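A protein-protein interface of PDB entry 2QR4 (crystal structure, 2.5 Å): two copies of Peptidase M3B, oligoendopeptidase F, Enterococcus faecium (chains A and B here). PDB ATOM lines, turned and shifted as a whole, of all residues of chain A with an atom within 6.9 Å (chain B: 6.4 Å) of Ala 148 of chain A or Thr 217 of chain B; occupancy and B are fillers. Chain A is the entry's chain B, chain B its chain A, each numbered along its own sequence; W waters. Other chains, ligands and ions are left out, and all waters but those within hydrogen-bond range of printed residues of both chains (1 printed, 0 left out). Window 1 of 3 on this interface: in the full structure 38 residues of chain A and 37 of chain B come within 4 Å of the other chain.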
ATOM      1  N   GLY A 143      14.963   1.369 -26.288  1.00  0.00           N
ATOM      2  CA  GLY A 143      15.343   0.593 -25.100  1.00  0.00           C
ATOM      3  C   GLY A 143      16.401   1.278 -24.257  1.00  0.00           C
ATOM      4  O   GLY A 143      16.296   1.352 -23.031  1.00  0.00           O
ATOM      5  N   GLU A 144      17.411   1.803 -24.935  1.00  0.00           N
ATOM      6  CA  GLU A 144      18.522   2.506 -24.302  1.00  0.00           C
ATOM      7  C   GLU A 144      18.008   3.778 -23.622  1.00  0.00           C
ATOM      8  O   GLU A 144      18.427   4.109 -22.519  1.00  0.00           O
ATOM      9  CB  GLU A 144      19.550   2.856 -25.380  1.00  0.00           C
ATOM     10  CG  GLU A 144      20.991   2.700 -25.029  1.00  0.00           C
ATOM     11  CD  GLU A 144      21.856   2.694 -26.272  1.00  0.00           C
ATOM     12  OE1 GLU A 144      21.315   2.384 -27.347  1.00  0.00           O
ATOM     13  OE2 GLU A 144      23.064   2.993 -26.187  1.00  0.00           O
ATOM     14  N   ILE A 145      17.100   4.499 -24.277  1.00  0.00           N
ATOM     15  CA  ILE A 145      16.516   5.684 -23.647  1.00  0.00           C
ATOM     16  C   ILE A 145      15.766   5.306 -22.354  1.00  0.00           C
ATOM     17  O   ILE A 145      15.852   6.013 -21.355  1.00  0.00           O
ATOM     18  CB  ILE A 145      15.558   6.449 -24.591  1.00  0.00           C
ATOM     19  CG1 ILE A 145      16.219   6.749 -25.945  1.00  0.00           C
ATOM     20  CG2 ILE A 145      15.020   7.705 -23.904  1.00  0.00           C
ATOM     21  CD1 ILE A 145      17.506   7.470 -25.830  1.00  0.00           C
ATOM     22  N   PHE A 146      15.048   4.186 -22.359  1.00  0.00           N
ATOM     23  CA  PHE A 146      14.296   3.763 -21.159  1.00  0.00           C
ATOM     24  C   PHE A 146      15.145   3.390 -19.948  1.00  0.00           C
ATOM     25  O   PHE A 146      14.698   3.535 -18.815  1.00  0.00           O
ATOM     26  CB  PHE A 146      13.341   2.600 -21.477  1.00  0.00           C
ATOM     27  CG  PHE A 146      12.071   3.031 -22.162  1.00  0.00           C
ATOM     28  CD1 PHE A 146      11.894   2.821 -23.518  1.00  0.00           C
ATOM     29  CD2 PHE A 146      11.064   3.652 -21.448  1.00  0.00           C
ATOM     30  CE1 PHE A 146      10.733   3.222 -24.153  1.00  0.00           C
ATOM     31  CE2 PHE A 146       9.897   4.058 -22.076  1.00  0.00           C
ATOM     32  CZ  PHE A 146       9.732   3.844 -23.432  1.00  0.00           C
ATOM     33  N   ASP A 147      16.360   2.895 -20.138  1.00  0.00           N
ATOM     34  CA  ASP A 147      17.128   2.600 -18.926  1.00  0.00           C
ATOM     35  C   ASP A 147      18.357   3.477 -18.744  1.00  0.00           C
ATOM     36  O   ASP A 147      19.240   3.172 -17.949  1.00  0.00           O
ATOM     37  CB  ASP A 147      17.436   1.114 -18.803  1.00  0.00           C
ATOM     38  CG  ASP A 147      17.686   0.493 -20.120  1.00  0.00           C
ATOM     39  OD1 ASP A 147      17.111  -0.578 -20.390  1.00  0.00           O
ATOM     40  OD2 ASP A 147      18.434   1.116 -20.898  1.00  0.00           O
ATOM     41  N   ALA A 148      18.347   4.605 -19.447  1.00  0.00           N
ATOM     42  CA  ALA A 148      19.385   5.612 -19.357  1.00  0.00           C
ATOM     43  C   ALA A 148      19.567   6.065 -17.919  1.00  0.00           C
ATOM     44  O   ALA A 148      20.698   6.197 -17.432  1.00  0.00           O
ATOM     45  CB  ALA A 148      19.015   6.818 -20.233  1.00  0.00           C
ATOM     46  N   SER A 149      18.454   6.318 -17.239  1.00  0.00           N
ATOM     47  CA  SER A 149      18.517   6.811 -15.854  1.00  0.00           C
ATOM     48  C   SER A 149      19.145   5.790 -14.891  1.00  0.00           C
ATOM     49  O   SER A 149      19.815   6.180 -13.941  1.00  0.00           O
ATOM     50  CB  SER A 149      17.147   7.298 -15.350  1.00  0.00           C
ATOM     51  OG  SER A 149      16.276   6.208 -15.115  1.00  0.00           O
ATOM     52  N   SER A 150      18.958   4.496 -15.144  1.00  0.00           N
ATOM     53  CA  SER A 150      19.709   3.492 -14.391  1.00  0.00           C
ATOM     54  C   SER A 150      21.192   3.663 -14.665  1.00  0.00           C
ATOM     55  O   SER A 150      22.021   3.527 -13.756  1.00  0.00           O
ATOM     56  CB  SER A 150      19.316   2.068 -14.767  1.00  0.00           C
ATOM     57  OG  SER A 150      17.982   1.809 -14.413  1.00  0.00           O
ATOM     58  N   ASP A 151      21.539   3.934 -15.922  1.00  0.00           N
ATOM     59  CA  ASP A 151      22.963   4.124 -16.269  1.00  0.00           C
ATOM     60  C   ASP A 151      23.504   5.365 -15.548  1.00  0.00           C
ATOM     61  O   ASP A 151      24.569   5.328 -14.949  1.00  0.00           O
ATOM     62  CB  ASP A 151      23.159   4.243 -17.783  1.00  0.00           C
ATOM     63  CG  ASP A 151      22.800   2.957 -18.540  1.00  0.00           C
ATOM     64  OD1 ASP A 151      22.951   1.857 -17.980  1.00  0.00           O
ATOM     65  OD2 ASP A 151      22.385   3.049 -19.713  1.00  0.00           O
ATOM     66  N   THR A 152      22.706   6.435 -15.533  1.00  0.00           N
ATOM     67  CA  THR A 152      23.089   7.673 -14.862  1.00  0.00           C
ATOM     68  C   THR A 152      23.260   7.462 -13.377  1.00  0.00           C
ATOM     69  O   THR A 152      24.248   7.914 -12.802  1.00  0.00           O
ATOM     70  CB  THR A 152      22.080   8.775 -15.129  1.00  0.00           C
ATOM     71  OG1 THR A 152      21.941   8.914 -16.544  1.00  0.00           O
ATOM     72  CG2 THR A 152      22.553  10.108 -14.523  1.00  0.00           C
ATOM     73  N   PHE A 153      22.325   6.746 -12.759  1.00  0.00           N
ATOM     74  CA  PHE A 153      22.501   6.366 -11.368  1.00  0.00           C
ATOM     75  C   PHE A 153      23.884   5.734 -11.122  1.00  0.00           C
ATOM     76  O   PHE A 153      24.606   6.135 -10.207  1.00  0.00           O
ATOM     77  CB  PHE A 153      21.438   5.364 -10.940  1.00  0.00           C
ATOM     78  CG  PHE A 153      21.694   4.772  -9.579  1.00  0.00           C
ATOM     79  CD1 PHE A 153      21.531   5.538  -8.438  1.00  0.00           C
ATOM     80  CD2 PHE A 153      22.119   3.462  -9.442  1.00  0.00           C
ATOM     81  CE1 PHE A 153      21.768   5.003  -7.185  1.00  0.00           C
ATOM     82  CE2 PHE A 153      22.371   2.925  -8.186  1.00  0.00           C
ATOM     83  CZ  PHE A 153      22.192   3.705  -7.058  1.00  0.00           C
ATOM     84  N   ALA A 154      24.249   4.741 -11.936  1.00  0.00           N
ATOM     85  CA  ALA A 154      25.449   3.959 -11.657  1.00  0.00           C
ATOM     86  C   ALA A 154      26.699   4.823 -11.729  1.00  0.00           C
ATOM     87  O   ALA A 154      27.568   4.715 -10.865  1.00  0.00           O
ATOM     88  CB  ALA A 154      25.571   2.761 -12.610  1.00  0.00           C
ATOM     89  N   THR A 214      16.535  10.556 -11.199  1.00  0.00           N
ATOM     90  CA  THR A 214      16.883   9.294 -11.880  1.00  0.00           C
ATOM     91  C   THR A 214      15.958   8.126 -11.481  1.00  0.00           C
ATOM     92  O   THR A 214      15.502   7.373 -12.340  1.00  0.00           O
ATOM     93  CB  THR A 214      18.369   8.893 -11.706  1.00  0.00           C
ATOM     94  OG1 THR A 214      18.633   8.615 -10.327  1.00  0.00           O
ATOM     95  CG2 THR A 214      19.311  10.013 -12.194  1.00  0.00           C
ATOM     96  N   THR A 217      12.350   8.700 -12.852  1.00  0.00           N
ATOM     97  CA  THR A 217      12.336   8.421 -14.276  1.00  0.00           C
ATOM     98  C   THR A 217      12.269   6.913 -14.534  1.00  0.00           C
ATOM     99  O   THR A 217      11.515   6.463 -15.390  1.00  0.00           O
ATOM    100  CB  THR A 217      13.545   9.059 -14.954  1.00  0.00           C
ATOM    101  OG1 THR A 217      13.454  10.475 -14.780  1.00  0.00           O
ATOM    102  CG2 THR A 217      13.578   8.729 -16.448  1.00  0.00           C
ATOM    103  N   HIS A 218      13.028   6.147 -13.758  1.00  0.00           N
ATOM    104  CA  HIS A 218      13.023   4.692 -13.848  1.00  0.00           C
ATOM    105  C   HIS A 218      11.649   4.107 -13.550  1.00  0.00           C
ATOM    106  O   HIS A 218      11.162   3.243 -14.273  1.00  0.00           O
ATOM    107  CB  HIS A 218      14.037   4.085 -12.876  1.00  0.00           C
ATOM    108  CG  HIS A 218      14.237   2.615 -13.067  1.00  0.00           C
ATOM    109  ND1 HIS A 218      14.913   2.092 -14.153  1.00  0.00           N
ATOM    110  CD2 HIS A 218      13.831   1.555 -12.327  1.00  0.00           C
ATOM    111  CE1 HIS A 218      14.936   0.774 -14.060  1.00  0.00           C
ATOM    112  NE2 HIS A 218      14.286   0.421 -12.965  1.00  0.00           N
ATOM    113  N   ILE B 145       9.778  10.418 -20.559  1.00  0.00           N
ATOM    114  CA  ILE B 145      10.998   9.634 -20.563  1.00  0.00           C
ATOM    115  C   ILE B 145      12.064  10.303 -21.445  1.00  0.00           C
ATOM    116  O   ILE B 145      13.184  10.513 -21.002  1.00  0.00           O
ATOM    117  CB  ILE B 145      10.742   8.197 -21.031  1.00  0.00           C
ATOM    118  CG1 ILE B 145       9.550   7.589 -20.291  1.00  0.00           C
ATOM    119  CG2 ILE B 145      11.973   7.363 -20.861  1.00  0.00           C
ATOM    120  CD1 ILE B 145       9.571   7.777 -18.807  1.00  0.00           C
ATOM    121  N   PHE B 146      11.718  10.692 -22.671  1.00  0.00           N
ATOM    122  CA  PHE B 146      12.723  11.362 -23.534  1.00  0.00           C
ATOM    123  C   PHE B 146      13.317  12.635 -22.938  1.00  0.00           C
ATOM    124  O   PHE B 146      14.507  12.895 -23.090  1.00  0.00           O
ATOM    125  CB  PHE B 146      12.175  11.647 -24.933  1.00  0.00           C
ATOM    126  CG  PHE B 146      11.994  10.419 -25.750  1.00  0.00           C
ATOM    127  CD1 PHE B 146      10.761   9.820 -25.852  1.00  0.00           C
ATOM    128  CD2 PHE B 146      13.069   9.841 -26.386  1.00  0.00           C
ATOM    129  CE1 PHE B 146      10.599   8.664 -26.584  1.00  0.00           C
ATOM    130  CE2 PHE B 146      12.911   8.681 -27.119  1.00  0.00           C
ATOM    131  CZ  PHE B 146      11.678   8.090 -27.214  1.00  0.00           C
ATOM    132  N   SER B 149      16.294  13.379 -18.851  1.00  0.00           N
ATOM    133  CA  SER B 149      17.696  13.685 -18.567  1.00  0.00           C
ATOM    134  C   SER B 149      18.026  15.193 -18.595  1.00  0.00           C
ATOM    135  O   SER B 149      18.991  15.605 -17.972  1.00  0.00           O
ATOM    136  CB  SER B 149      18.627  12.895 -19.485  1.00  0.00           C
ATOM    137  OG  SER B 149      18.688  13.485 -20.777  1.00  0.00           O
ATOM    138  N   ALA B 212      27.965  13.618 -18.932  1.00  0.00           N
ATOM    139  CA  ALA B 212      28.075  12.931 -20.220  1.00  0.00           C
ATOM    140  C   ALA B 212      26.878  12.004 -20.397  1.00  0.00           C
ATOM    141  O   ALA B 212      26.301  11.905 -21.472  1.00  0.00           O
ATOM    142  CB  ALA B 212      29.364  12.126 -20.292  1.00  0.00           C
ATOM    143  N   SER B 213      26.534  11.320 -19.319  1.00  0.00           N
ATOM    144  CA  SER B 213      25.409  10.424 -19.288  1.00  0.00           C
ATOM    145  C   SER B 213      24.109  11.185 -19.562  1.00  0.00           C
ATOM    146  O   SER B 213      23.332  10.787 -20.425  1.00  0.00           O
ATOM    147  CB  SER B 213      25.363   9.703 -17.931  1.00  0.00           C
ATOM    148  OG  SER B 213      24.226   8.858 -17.831  1.00  0.00           O
ATOM    149  N   THR B 214      23.873  12.285 -18.851  1.00  0.00           N
ATOM    150  CA  THR B 214      22.611  13.048 -19.060  1.00  0.00           C
ATOM    151  C   THR B 214      22.551  13.652 -20.455  1.00  0.00           C
ATOM    152  O   THR B 214      21.528  13.567 -21.125  1.00  0.00           O
ATOM    153  CB  THR B 214      22.356  14.151 -17.985  1.00  0.00           C
ATOM    154  OG1 THR B 214      23.515  14.991 -17.843  1.00  0.00           O
ATOM    155  CG2 THR B 214      22.042  13.518 -16.633  1.00  0.00           C
ATOM    156  N   LEU B 215      23.665  14.221 -20.913  1.00  0.00           N
ATOM    157  CA  LEU B 215      23.688  14.889 -22.218  1.00  0.00           C
ATOM    158  C   LEU B 215      23.653  13.869 -23.348  1.00  0.00           C
ATOM    159  O   LEU B 215      22.879  14.003 -24.291  1.00  0.00           O
ATOM    160  CB  LEU B 215      24.901  15.808 -22.345  1.00  0.00           C
ATOM    161  CG  LEU B 215      25.047  16.572 -23.658  1.00  0.00           C
ATOM    162  CD1 LEU B 215      23.763  17.379 -24.007  1.00  0.00           C
ATOM    163  CD2 LEU B 215      26.283  17.465 -23.622  1.00  0.00           C
ATOM    164  N   GLY B 216      24.490  12.842 -23.231  1.00  0.00           N
ATOM    165  CA  GLY B 216      24.428  11.669 -24.104  1.00  0.00           C
ATOM    166  C   GLY B 216      23.032  11.088 -24.311  1.00  0.00           C
ATOM    167  O   GLY B 216      22.624  10.806 -25.444  1.00  0.00           O
ATOM    168  N   THR B 217      22.284  10.912 -23.226  1.00  0.00           N
ATOM    169  CA  THR B 217      20.911  10.415 -23.339  1.00  0.00           C
ATOM    170  C   THR B 217      20.038  11.375 -24.166  1.00  0.00           C
ATOM    171  O   THR B 217      19.254  10.955 -25.025  1.00  0.00           O
ATOM    172  CB  THR B 217      20.296  10.225 -21.958  1.00  0.00           C
ATOM    173  OG1 THR B 217      21.107   9.312 -21.197  1.00  0.00           O
ATOM    174  CG2 THR B 217      18.891   9.676 -22.091  1.00  0.00           C
ATOM    175  N   HIS B 218      20.202  12.668 -23.905  1.00  0.00           N
ATOM    176  CA  HIS B 218      19.428  13.706 -24.580  1.00  0.00           C
ATOM    177  C   HIS B 218      19.693  13.634 -26.066  1.00  0.00           C
ATOM    178  O   HIS B 218      18.768  13.680 -26.875  1.00  0.00           O
ATOM    179  CB  HIS B 218      19.833  15.104 -24.069  1.00  0.00           C
ATOM    180  CG  HIS B 218      18.988  16.206 -24.608  1.00  0.00           C
ATOM    181  ND1 HIS B 218      17.665  16.368 -24.244  1.00  0.00           N
ATOM    182  CD2 HIS B 218      19.271  17.212 -25.469  1.00  0.00           C
ATOM    183  CE1 HIS B 218      17.169  17.426 -24.863  1.00  0.00           C
ATOM    184  NE2 HIS B 218      18.121  17.954 -25.614  1.00  0.00           N
ATOM    185  N   ILE B 219      20.975  13.522 -26.411  1.00  0.00           N
ATOM    186  CA  ILE B 219      21.413  13.423 -27.804  1.00  0.00           C
ATOM    187  C   ILE B 219      20.899  12.147 -28.488  1.00  0.00           C
ATOM    188  O   ILE B 219      20.364  12.202 -29.598  1.00  0.00           O
ATOM    189  CB  ILE B 219      22.934  13.563 -27.877  1.00  0.00           C
ATOM    190  CG1 ILE B 219      23.298  15.049 -27.731  1.00  0.00           C
ATOM    191  CG2 ILE B 219      23.470  13.000 -29.161  1.00  0.00           C
ATOM    192  CD1 ILE B 219      24.696  15.240 -27.317  1.00  0.00           C
ATOM    193  N   LYS B 220      21.011  11.014 -27.796  1.00  0.00           N
ATOM    194  CA  LYS B 220      20.415   9.768 -28.255  1.00  0.00           C
ATOM    195  C   LYS B 220      18.930   9.888 -28.611  1.00  0.00           C
ATOM    196  O   LYS B 220      18.487   9.337 -29.615  1.00  0.00           O
ATOM    197  CB  LYS B 220      20.615   8.658 -27.213  1.00  0.00           C
ATOM    198  CG  LYS B 220      21.795   7.801 -27.519  1.00  0.00           C
ATOM    199  CD  LYS B 220      22.134   6.809 -26.399  1.00  0.00           C
ATOM    200  CE  LYS B 220      23.563   6.325 -26.563  1.00  0.00           C
ATOM    201  NZ  LYS B 220      23.890   6.208 -28.039  1.00  0.00           N
ATOM    202  N   GLY B 221      18.165  10.603 -27.791  1.00  0.00           N
ATOM    203  CA  GLY B 221      16.722  10.792 -28.053  1.00  0.00           C
ATOM    204  C   GLY B 221      16.439  11.562 -29.329  1.00  0.00           C
ATOM    205  O   GLY B 221      15.516  11.203 -30.076  1.00  0.00           O
ATOM    206  N   HIS B 222      17.224  12.618 -29.588  1.00  0.00           N
ATOM    207  CA  HIS B 222      17.116  13.361 -30.851  1.00  0.00           C
ATOM    208  C   HIS B 222      17.392  12.472 -32.061  1.00  0.00           C
ATOM    209  O   HIS B 222      16.688  12.533 -33.067  1.00  0.00           O
ATOM    210  CB  HIS B 222      18.090  14.537 -30.892  1.00  0.00           C
ATOM    211  CG  HIS B 222      17.767  15.623 -29.922  1.00  0.00           C
ATOM    212  ND1 HIS B 222      18.686  16.583 -29.552  1.00  0.00           N
ATOM    213  CD2 HIS B 222      16.633  15.895 -29.233  1.00  0.00           C
ATOM    214  CE1 HIS B 222      18.127  17.403 -28.682  1.00  0.00           C
ATOM    215  NE2 HIS B 222      16.882  17.010 -28.473  1.00  0.00           N
HETATM  216  O   HOH W   1      20.067  10.170 -18.277  1.00  0.00           O
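The side-chain hydroxyl of Ser 213 of chain B sits at hydrogen-bond distance from the side-chain hydroxyl of Thr 152 of chain A (2.6 Å).
OE2 of Glu 144 of chain A lies within salt-bridge range of NZ of Lys 220 of chain B.
The backbone carbonyl oxygen of Ser 213 of chain B sits at hydrogen-bond distance from the side-chain hydroxyl of Thr 217 of chain B, 2.8 Å away.
O of Ala 148 of chain A sits at hydrogen-bond distance from OG1 of Thr 152 of chain A.
Among the printed residues, merely in contact across the chains: Ala 148 of chain A with Thr 217 of chain B (3.4 Å), Ile 145 of chain A with Lys 220 of chain B (3.6 Å), Ile 145 of chain A with Gly 221 of chain B (3.8 Å), Ile 145 of chain A with Phe 146 of chain B (3.8 Å), Phe 146 of chain A with Ile 145 of chain B (3.9 Å) and Ile 145 of chain A with Thr 217 of chain B (3.98 Å).
Ala 148 of chain A touches just one residue of chain B: Thr 217 (3.4 Å).
Printed residues of chain A within 4 Å of Thr 217 of chain B: Ile 145 (3.98 Å) and Ala 148 (3.4 Å).
Of the printed residues of chain A, Ser 213 of chain B touches Thr 152 (2.6 Å).
Printed residues of chain A within 4 Å of Ile 145 of chain B: Phe 146 (3.9 Å).
The nearest residue of chain B that does not touch Ala 148 of chain A is Ser 213 of chain B (4.4 Å).
The nearest printed residue of chain A that does not touch Ser 213 of chain B is Asp 151 of chain A (4.2 Å).
Hydrophobic or aromatic side chains of chain B that line the printed part of chain A: Ile 145 and Phe 146.
Among the printed residues, 8 pairs touch across the chains.
Ile 145 of chain A touches Phe 146 of chain B, and with the chains exchanged Phe 146 of chain A touches Ile 145 of chain B.
Ile 145 of chain A touches Thr 217 of chain B, but with the chains exchanged Thr 217 of chain A does not touch Ile 145 of chain B (4.1 Å).
Positions printed for both chains: 145, 146, 149, 214, 217 and 218.
Of the 8 pairs that touch across the chains among the printed residues, 2 have their exchanged pair printed and touching as well.
Water W1 lies within hydrogen-bond range of the side-chain hydroxyl (OG1) of Thr 152 of chain A and the side-chain hydroxyl (OG1) of Thr 217 of chain B.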
